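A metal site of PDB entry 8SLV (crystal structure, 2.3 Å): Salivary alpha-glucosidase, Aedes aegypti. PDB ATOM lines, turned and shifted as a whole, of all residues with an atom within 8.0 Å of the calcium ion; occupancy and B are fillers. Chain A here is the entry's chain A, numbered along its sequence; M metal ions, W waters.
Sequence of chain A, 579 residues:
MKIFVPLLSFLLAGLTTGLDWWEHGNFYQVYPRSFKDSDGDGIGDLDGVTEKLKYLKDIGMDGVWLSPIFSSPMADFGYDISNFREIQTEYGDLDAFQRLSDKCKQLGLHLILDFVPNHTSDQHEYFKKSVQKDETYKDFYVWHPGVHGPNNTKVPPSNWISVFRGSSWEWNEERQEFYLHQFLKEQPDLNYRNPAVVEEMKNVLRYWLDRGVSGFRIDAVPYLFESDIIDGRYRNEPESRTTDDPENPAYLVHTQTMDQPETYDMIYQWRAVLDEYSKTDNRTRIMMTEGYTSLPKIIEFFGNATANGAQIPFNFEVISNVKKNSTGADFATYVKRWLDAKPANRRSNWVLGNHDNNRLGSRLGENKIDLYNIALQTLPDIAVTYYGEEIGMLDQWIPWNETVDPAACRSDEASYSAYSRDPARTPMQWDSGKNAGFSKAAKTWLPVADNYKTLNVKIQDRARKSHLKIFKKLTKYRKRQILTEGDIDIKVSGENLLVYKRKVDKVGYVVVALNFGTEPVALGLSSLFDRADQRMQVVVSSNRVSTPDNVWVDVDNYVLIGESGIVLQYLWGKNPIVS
The side-chain carboxylate (OD1) of Asp 189 sits at hydrogen-bond distance from the backbone NH (N) of Gln 182, at 2.6 Å. The backbone carbonyl oxygen (O) of Leu 180 lies within hydrogen-bond range of the backbone NH (N) of Asp 189, at 3.1 Å. The side-chain amide oxygen (OE1) of Gln 182 sits close to the side-chain carboxylate (OE2) of Glu 226. The backbone NH (N) of Leu 190 sits at hydrogen-bond distance from the backbone carbonyl oxygen (O) of Asn 118. The side-chain amide nitrogen (ND2) of Asn 118 lies within hydrogen-bond range of a ring nitrogen (ND1) of His 119.
Along chain A the residues within 4 Å of the calcium ion span positions 118 to 226.
The calcium ion is bound by OD2 of Asp 189 (2.4 Å), O of Leu 224 (2.4 Å), OE2 of Glu 226 (2.4 Å), water W1 (2.5 Å), O of Tyr 223 (2.5 Å), water W2 (2.5 Å) and OD1 of Asn 118 (2.5 Å). The calcium ion has seven donor atoms within binding distance.
Water W1 lies within hydrogen-bond range of the backbone carbonyl oxygen of Asn 118 (2.7 Å) and the backbone carbonyl oxygen of Leu 190 (2.8 Å). Water W2 lies within hydrogen-bond range of OE1 of Glu 226 (2.6 Å) and O of Leu 190 (2.9 Å).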
ATOM      1  N   PRO A 117      10.085 -33.477  21.501  1.00  0.00           N
ATOM      2  CA  PRO A 117       9.997 -32.015  21.338  1.00  0.00           C
ATOM      3  C   PRO A 117       8.905 -31.348  22.143  1.00  0.00           C
ATOM      4  O   PRO A 117       8.951 -30.126  22.323  1.00  0.00           O
ATOM      5  CB  PRO A 117       9.718 -31.841  19.842  1.00  0.00           C
ATOM      6  CG  PRO A 117       8.921 -33.087  19.485  1.00  0.00           C
ATOM      7  CD  PRO A 117       9.545 -34.204  20.336  1.00  0.00           C
ATOM      8  N   ASN A 118       7.905 -32.086  22.614  1.00  0.00           N
ATOM      9  CA  ASN A 118       6.735 -31.382  23.111  1.00  0.00           C
ATOM     10  C   ASN A 118       7.024 -30.626  24.391  1.00  0.00           C
ATOM     11  O   ASN A 118       6.366 -29.622  24.673  1.00  0.00           O
ATOM     12  CB  ASN A 118       5.577 -32.338  23.358  1.00  0.00           C
ATOM     13  CG  ASN A 118       4.343 -31.598  23.752  1.00  0.00           C
ATOM     14  OD1 ASN A 118       3.773 -30.865  22.930  1.00  0.00           O
ATOM     15  ND2 ASN A 118       3.936 -31.734  25.014  1.00  0.00           N
ATOM     16  N   HIS A 119       7.995 -31.088  25.173  1.00  0.00           N
ATOM     17  CA  HIS A 119       8.177 -30.575  26.533  1.00  0.00           C
ATOM     18  C   HIS A 119       9.609 -30.823  26.951  1.00  0.00           C
ATOM     19  O   HIS A 119      10.316 -31.657  26.379  1.00  0.00           O
ATOM     20  CB  HIS A 119       7.216 -31.260  27.503  1.00  0.00           C
ATOM     21  CG  HIS A 119       7.145 -32.745  27.309  1.00  0.00           C
ATOM     22  ND1 HIS A 119       6.187 -33.351  26.510  1.00  0.00           N
ATOM     23  CD2 HIS A 119       7.945 -33.743  27.757  1.00  0.00           C
ATOM     24  CE1 HIS A 119       6.388 -34.654  26.503  1.00  0.00           C
ATOM     25  NE2 HIS A 119       7.453 -34.929  27.243  1.00  0.00           N
ATOM     26  N   VAL A 142       4.523 -22.029  27.502  1.00  0.00           N
ATOM     27  CA  VAL A 142       3.181 -21.508  27.253  1.00  0.00           C
ATOM     28  C   VAL A 142       2.631 -21.031  28.588  1.00  0.00           C
ATOM     29  O   VAL A 142       2.164 -21.833  29.407  1.00  0.00           O
ATOM     30  CB  VAL A 142       2.275 -22.540  26.589  1.00  0.00           C
ATOM     31  CG1 VAL A 142       0.953 -21.903  26.260  1.00  0.00           C
ATOM     32  CG2 VAL A 142       2.946 -23.117  25.316  1.00  0.00           C
ATOM     33  N   LEU A 180       1.561 -24.273  30.711  1.00  0.00           N
ATOM     34  CA  LEU A 180       0.909 -25.431  30.117  1.00  0.00           C
ATOM     35  C   LEU A 180       1.731 -26.721  30.282  1.00  0.00           C
ATOM     36  O   LEU A 180       2.919 -26.693  30.107  1.00  0.00           O
ATOM     37  CB  LEU A 180       0.598 -25.129  28.660  1.00  0.00           C
ATOM     38  CG  LEU A 180      -0.104 -26.282  27.963  1.00  0.00           C
ATOM     39  CD1 LEU A 180      -1.564 -26.238  28.306  1.00  0.00           C
ATOM     40  CD2 LEU A 180       0.128 -26.275  26.484  1.00  0.00           C
ATOM     41  N   HIS A 181       1.075 -27.780  30.697  1.00  0.00           N
ATOM     42  CA  HIS A 181       1.701 -29.125  30.747  1.00  0.00           C
ATOM     43  C   HIS A 181       0.700 -30.124  30.190  1.00  0.00           C
ATOM     44  O   HIS A 181      -0.206 -30.476  30.851  1.00  0.00           O
ATOM     45  CB  HIS A 181       2.295 -29.465  32.116  1.00  0.00           C
ATOM     46  CG  HIS A 181       1.281 -29.613  33.196  1.00  0.00           C
ATOM     47  ND1 HIS A 181       0.883 -30.803  33.636  1.00  0.00           N
ATOM     48  CD2 HIS A 181       0.581 -28.714  33.874  1.00  0.00           C
ATOM     49  CE1 HIS A 181      -0.023 -30.653  34.545  1.00  0.00           C
ATOM     50  NE2 HIS A 181      -0.214 -29.386  34.718  1.00  0.00           N
ATOM     51  N   GLN A 182       0.901 -30.562  28.980  1.00  0.00           N
ATOM     52  CA  GLN A 182      -0.005 -31.590  28.440  1.00  0.00           C
ATOM     53  C   GLN A 182       0.254 -32.942  29.098  1.00  0.00           C
ATOM     54  O   GLN A 182      -0.628 -33.685  29.171  1.00  0.00           O
ATOM     55  CB  GLN A 182      -0.041 -31.581  26.927  1.00  0.00           C
ATOM     56  CG  GLN A 182      -0.961 -30.475  26.450  1.00  0.00           C
ATOM     57  CD  GLN A 182      -1.868 -30.828  25.312  1.00  0.00           C
ATOM     58  OE1 GLN A 182      -1.587 -30.517  24.198  1.00  0.00           O
ATOM     59  NE2 GLN A 182      -2.992 -31.432  25.596  1.00  0.00           N
ATOM     60  N   PHE A 183       1.463 -33.148  29.591  1.00  0.00           N
ATOM     61  CA  PHE A 183       1.833 -34.387  30.302  1.00  0.00           C
ATOM     62  C   PHE A 183       1.982 -34.079  31.794  1.00  0.00           C
ATOM     63  O   PHE A 183       1.102 -33.522  32.333  1.00  0.00           O
ATOM     64  CB  PHE A 183       2.883 -35.157  29.527  1.00  0.00           C
ATOM     65  CG  PHE A 183       2.453 -35.554  28.143  1.00  0.00           C
ATOM     66  CD1 PHE A 183       1.844 -36.776  27.907  1.00  0.00           C
ATOM     67  CD2 PHE A 183       2.656 -34.715  27.052  1.00  0.00           C
ATOM     68  CE1 PHE A 183       1.479 -37.145  26.630  1.00  0.00           C
ATOM     69  CE2 PHE A 183       2.288 -35.092  25.779  1.00  0.00           C
ATOM     70  CZ  PHE A 183       1.705 -36.313  25.562  1.00  0.00           C
ATOM     71  N   PRO A 188       6.865 -29.115  31.428  1.00  0.00           N
ATOM     72  CA  PRO A 188       6.328 -27.916  30.800  1.00  0.00           C
ATOM     73  C   PRO A 188       6.483 -27.962  29.267  1.00  0.00           C
ATOM     74  O   PRO A 188       7.504 -28.268  28.799  1.00  0.00           O
ATOM     75  CB  PRO A 188       7.109 -26.778  31.448  1.00  0.00           C
ATOM     76  CG  PRO A 188       8.342 -27.427  31.994  1.00  0.00           C
ATOM     77  CD  PRO A 188       7.907 -28.804  32.375  1.00  0.00           C
ATOM     78  N   ASP A 189       5.385 -27.701  28.581  1.00  0.00           N
ATOM     79  CA  ASP A 189       5.275 -27.675  27.104  1.00  0.00           C
ATOM     80  C   ASP A 189       6.079 -26.523  26.500  1.00  0.00           C
ATOM     81  O   ASP A 189       5.984 -25.419  26.952  1.00  0.00           O
ATOM     82  CB  ASP A 189       3.821 -27.541  26.651  1.00  0.00           C
ATOM     83  CG  ASP A 189       2.990 -28.799  26.509  1.00  0.00           C
ATOM     84  OD1 ASP A 189       2.767 -29.471  27.473  1.00  0.00           O
ATOM     85  OD2 ASP A 189       2.513 -29.009  25.481  1.00  0.00           O
ATOM     86  N   LEU A 190       6.857 -26.847  25.491  1.00  0.00           N
ATOM     87  CA  LEU A 190       7.586 -25.847  24.681  1.00  0.00           C
ATOM     88  C   LEU A 190       6.588 -25.060  23.818  1.00  0.00           C
ATOM     89  O   LEU A 190       5.645 -25.609  23.408  1.00  0.00           O
ATOM     90  CB  LEU A 190       8.633 -26.581  23.841  1.00  0.00           C
ATOM     91  CG  LEU A 190       9.938 -26.863  24.573  1.00  0.00           C
ATOM     92  CD1 LEU A 190      10.922 -27.553  23.662  1.00  0.00           C
ATOM     93  CD2 LEU A 190      10.499 -25.621  25.199  1.00  0.00           C
ATOM     94  N   ASN A 191       6.856 -23.773  23.619  1.00  0.00           N
ATOM     95  CA  ASN A 191       5.976 -22.880  22.879  1.00  0.00           C
ATOM     96  C   ASN A 191       6.478 -22.799  21.439  1.00  0.00           C
ATOM     97  O   ASN A 191       7.334 -21.979  21.116  1.00  0.00           O
ATOM     98  CB  ASN A 191       5.933 -21.507  23.547  1.00  0.00           C
ATOM     99  CG  ASN A 191       5.135 -20.505  22.757  1.00  0.00           C
ATOM    100  OD1 ASN A 191       4.233 -20.876  22.023  1.00  0.00           O
ATOM    101  ND2 ASN A 191       5.432 -19.231  22.927  1.00  0.00           N
ATOM    102  N   TYR A 192       5.942 -23.669  20.583  1.00  0.00           N
ATOM    103  CA  TYR A 192       6.395 -23.681  19.200  1.00  0.00           C
ATOM    104  C   TYR A 192       5.823 -22.538  18.366  1.00  0.00           C
ATOM    105  O   TYR A 192       6.085 -22.496  17.156  1.00  0.00           O
ATOM    106  CB  TYR A 192       6.078 -25.042  18.550  1.00  0.00           C
ATOM    107  CG  TYR A 192       7.080 -26.064  18.994  1.00  0.00           C
ATOM    108  CD1 TYR A 192       8.324 -26.150  18.386  1.00  0.00           C
ATOM    109  CD2 TYR A 192       6.816 -26.894  20.078  1.00  0.00           C
ATOM    110  CE1 TYR A 192       9.263 -27.061  18.824  1.00  0.00           C
ATOM    111  CE2 TYR A 192       7.745 -27.797  20.522  1.00  0.00           C
ATOM    112  CZ  TYR A 192       8.966 -27.876  19.890  1.00  0.00           C
ATOM    113  OH  TYR A 192       9.905 -28.786  20.329  1.00  0.00           O
ATOM    114  N   ALA A 220       4.941 -37.948  21.109  1.00  0.00           N
ATOM    115  CA  ALA A 220       3.727 -37.157  21.381  1.00  0.00           C
ATOM    116  C   ALA A 220       3.406 -36.137  20.286  1.00  0.00           C
ATOM    117  O   ALA A 220       3.042 -35.002  20.571  1.00  0.00           O
ATOM    118  CB  ALA A 220       3.846 -36.438  22.727  1.00  0.00           C
ATOM    119  N   VAL A 221       3.514 -36.545  19.022  1.00  0.00           N
ATOM    120  CA  VAL A 221       3.336 -35.563  17.961  1.00  0.00           C
ATOM    121  C   VAL A 221       1.964 -34.902  17.968  1.00  0.00           C
ATOM    122  O   VAL A 221       1.895 -33.704  17.664  1.00  0.00           O
ATOM    123  CB  VAL A 221       3.663 -36.170  16.575  1.00  0.00           C
ATOM    124  CG1 VAL A 221       5.165 -36.354  16.433  1.00  0.00           C
ATOM    125  CG2 VAL A 221       2.960 -37.489  16.341  1.00  0.00           C
ATOM    126  N   PRO A 222       0.845 -35.559  18.331  1.00  0.00           N
ATOM    127  CA  PRO A 222      -0.450 -34.849  18.268  1.00  0.00           C
ATOM    128  C   PRO A 222      -0.568 -33.640  19.180  1.00  0.00           C
ATOM    129  O   PRO A 222      -1.485 -32.833  18.986  1.00  0.00           O
ATOM    130  CB  PRO A 222      -1.482 -35.918  18.675  1.00  0.00           C
ATOM    131  CG  PRO A 222      -0.818 -37.203  18.375  1.00  0.00           C
ATOM    132  CD  PRO A 222       0.633 -36.975  18.699  1.00  0.00           C
ATOM    133  N   TYR A 223       0.307 -33.494  20.174  1.00  0.00           N
ATOM    134  CA  TYR A 223       0.157 -32.490  21.217  1.00  0.00           C
ATOM    135  C   TYR A 223       1.074 -31.289  21.054  1.00  0.00           C
ATOM    136  O   TYR A 223       1.164 -30.462  21.962  1.00  0.00           O
ATOM    137  CB  TYR A 223       0.400 -33.135  22.586  1.00  0.00           C
ATOM    138  CG  TYR A 223      -0.527 -34.277  22.930  1.00  0.00           C
ATOM    139  CD1 TYR A 223      -1.731 -34.061  23.590  1.00  0.00           C
ATOM    140  CD2 TYR A 223      -0.185 -35.591  22.608  1.00  0.00           C
ATOM    141  CE1 TYR A 223      -2.576 -35.100  23.913  1.00  0.00           C
ATOM    142  CE2 TYR A 223      -1.037 -36.634  22.920  1.00  0.00           C
ATOM    143  CZ  TYR A 223      -2.235 -36.382  23.580  1.00  0.00           C
ATOM    144  OH  TYR A 223      -3.085 -37.423  23.916  1.00  0.00           O
ATOM    145  N   LEU A 224       1.774 -31.180  19.924  1.00  0.00           N
ATOM    146  CA  LEU A 224       2.810 -30.160  19.755  1.00  0.00           C
ATOM    147  C   LEU A 224       2.255 -28.743  19.881  1.00  0.00           C
ATOM    148  O   LEU A 224       2.620 -28.005  20.812  1.00  0.00           O
ATOM    149  CB  LEU A 224       3.473 -30.350  18.410  1.00  0.00           C
ATOM    150  CG  LEU A 224       4.953 -30.022  18.402  1.00  0.00           C
ATOM    151  CD1 LEU A 224       5.688 -30.894  19.411  1.00  0.00           C
ATOM    152  CD2 LEU A 224       5.503 -30.224  17.004  1.00  0.00           C
ATOM    153  N   PHE A 225       1.395 -28.360  18.954  1.00  0.00           N
ATOM    154  CA  PHE A 225       0.747 -27.063  18.972  1.00  0.00           C
ATOM    155  C   PHE A 225      -0.612 -27.159  19.653  1.00  0.00           C
ATOM    156  O   PHE A 225      -1.349 -28.134  19.460  1.00  0.00           O
ATOM    157  CB  PHE A 225       0.546 -26.540  17.538  1.00  0.00           C
ATOM    158  CG  PHE A 225       1.732 -25.785  16.979  1.00  0.00           C
ATOM    159  CD1 PHE A 225       2.757 -26.448  16.334  1.00  0.00           C
ATOM    160  CD2 PHE A 225       1.802 -24.406  17.087  1.00  0.00           C
ATOM    161  CE1 PHE A 225       3.829 -25.748  15.791  1.00  0.00           C
ATOM    162  CE2 PHE A 225       2.863 -23.698  16.549  1.00  0.00           C
ATOM    163  CZ  PHE A 225       3.885 -24.369  15.909  1.00  0.00           C
ATOM    164  N   GLU A 226      -0.948 -26.144  20.434  1.00  0.00           N
ATOM    165  CA  GLU A 226      -2.325 -25.891  20.842  1.00  0.00           C
ATOM    166  C   GLU A 226      -2.836 -24.678  20.057  1.00  0.00           C
ATOM    167  O   GLU A 226      -2.040 -23.929  19.470  1.00  0.00           O
ATOM    168  CB  GLU A 226      -2.421 -25.644  22.352  1.00  0.00           C
ATOM    169  CG  GLU A 226      -1.899 -26.778  23.208  1.00  0.00           C
ATOM    170  CD  GLU A 226      -0.372 -26.876  23.196  1.00  0.00           C
ATOM    171  OE1 GLU A 226       0.307 -25.814  23.173  1.00  0.00           O
ATOM    172  OE2 GLU A 226       0.138 -28.002  23.236  1.00  0.00           O
ATOM    173  N   THR A 257      -6.303 -28.880  21.630  1.00  0.00           N
ATOM    174  CA  THR A 257      -5.028 -29.322  22.171  1.00  0.00           C
ATOM    175  C   THR A 257      -4.389 -30.465  21.409  1.00  0.00           C
ATOM    176  O   THR A 257      -3.269 -30.842  21.756  1.00  0.00           O
ATOM    177  CB  THR A 257      -5.195 -29.747  23.632  1.00  0.00           C
ATOM    178  OG1 THR A 257      -6.181 -30.778  23.719  1.00  0.00           O
ATOM    179  CG2 THR A 257      -5.618 -28.567  24.476  1.00  0.00           C
ATOM    180  N   THR A 263       0.868 -28.306  13.906  1.00  0.00           N
ATOM    181  CA  THR A 263       1.608 -29.508  14.291  1.00  0.00           C
ATOM    182  C   THR A 263       2.149 -30.230  13.060  1.00  0.00           C
ATOM    183  O   THR A 263       3.339 -30.597  12.999  1.00  0.00           O
ATOM    184  CB  THR A 263       0.700 -30.435  15.098  1.00  0.00           C
ATOM    185  OG1 THR A 263       0.382 -29.834  16.364  1.00  0.00           O
ATOM    186  CG2 THR A 263       1.361 -31.803  15.311  1.00  0.00           C
HETATM  187 CA    CA M   1       2.465 -28.702  23.130  1.00  0.00          CA
HETATM  188  O   HOH W   1       4.874 -28.228  22.920  1.00  0.00           O
HETATM  189  O   HOH W   2       2.790 -26.243  23.567  1.00  0.00           O
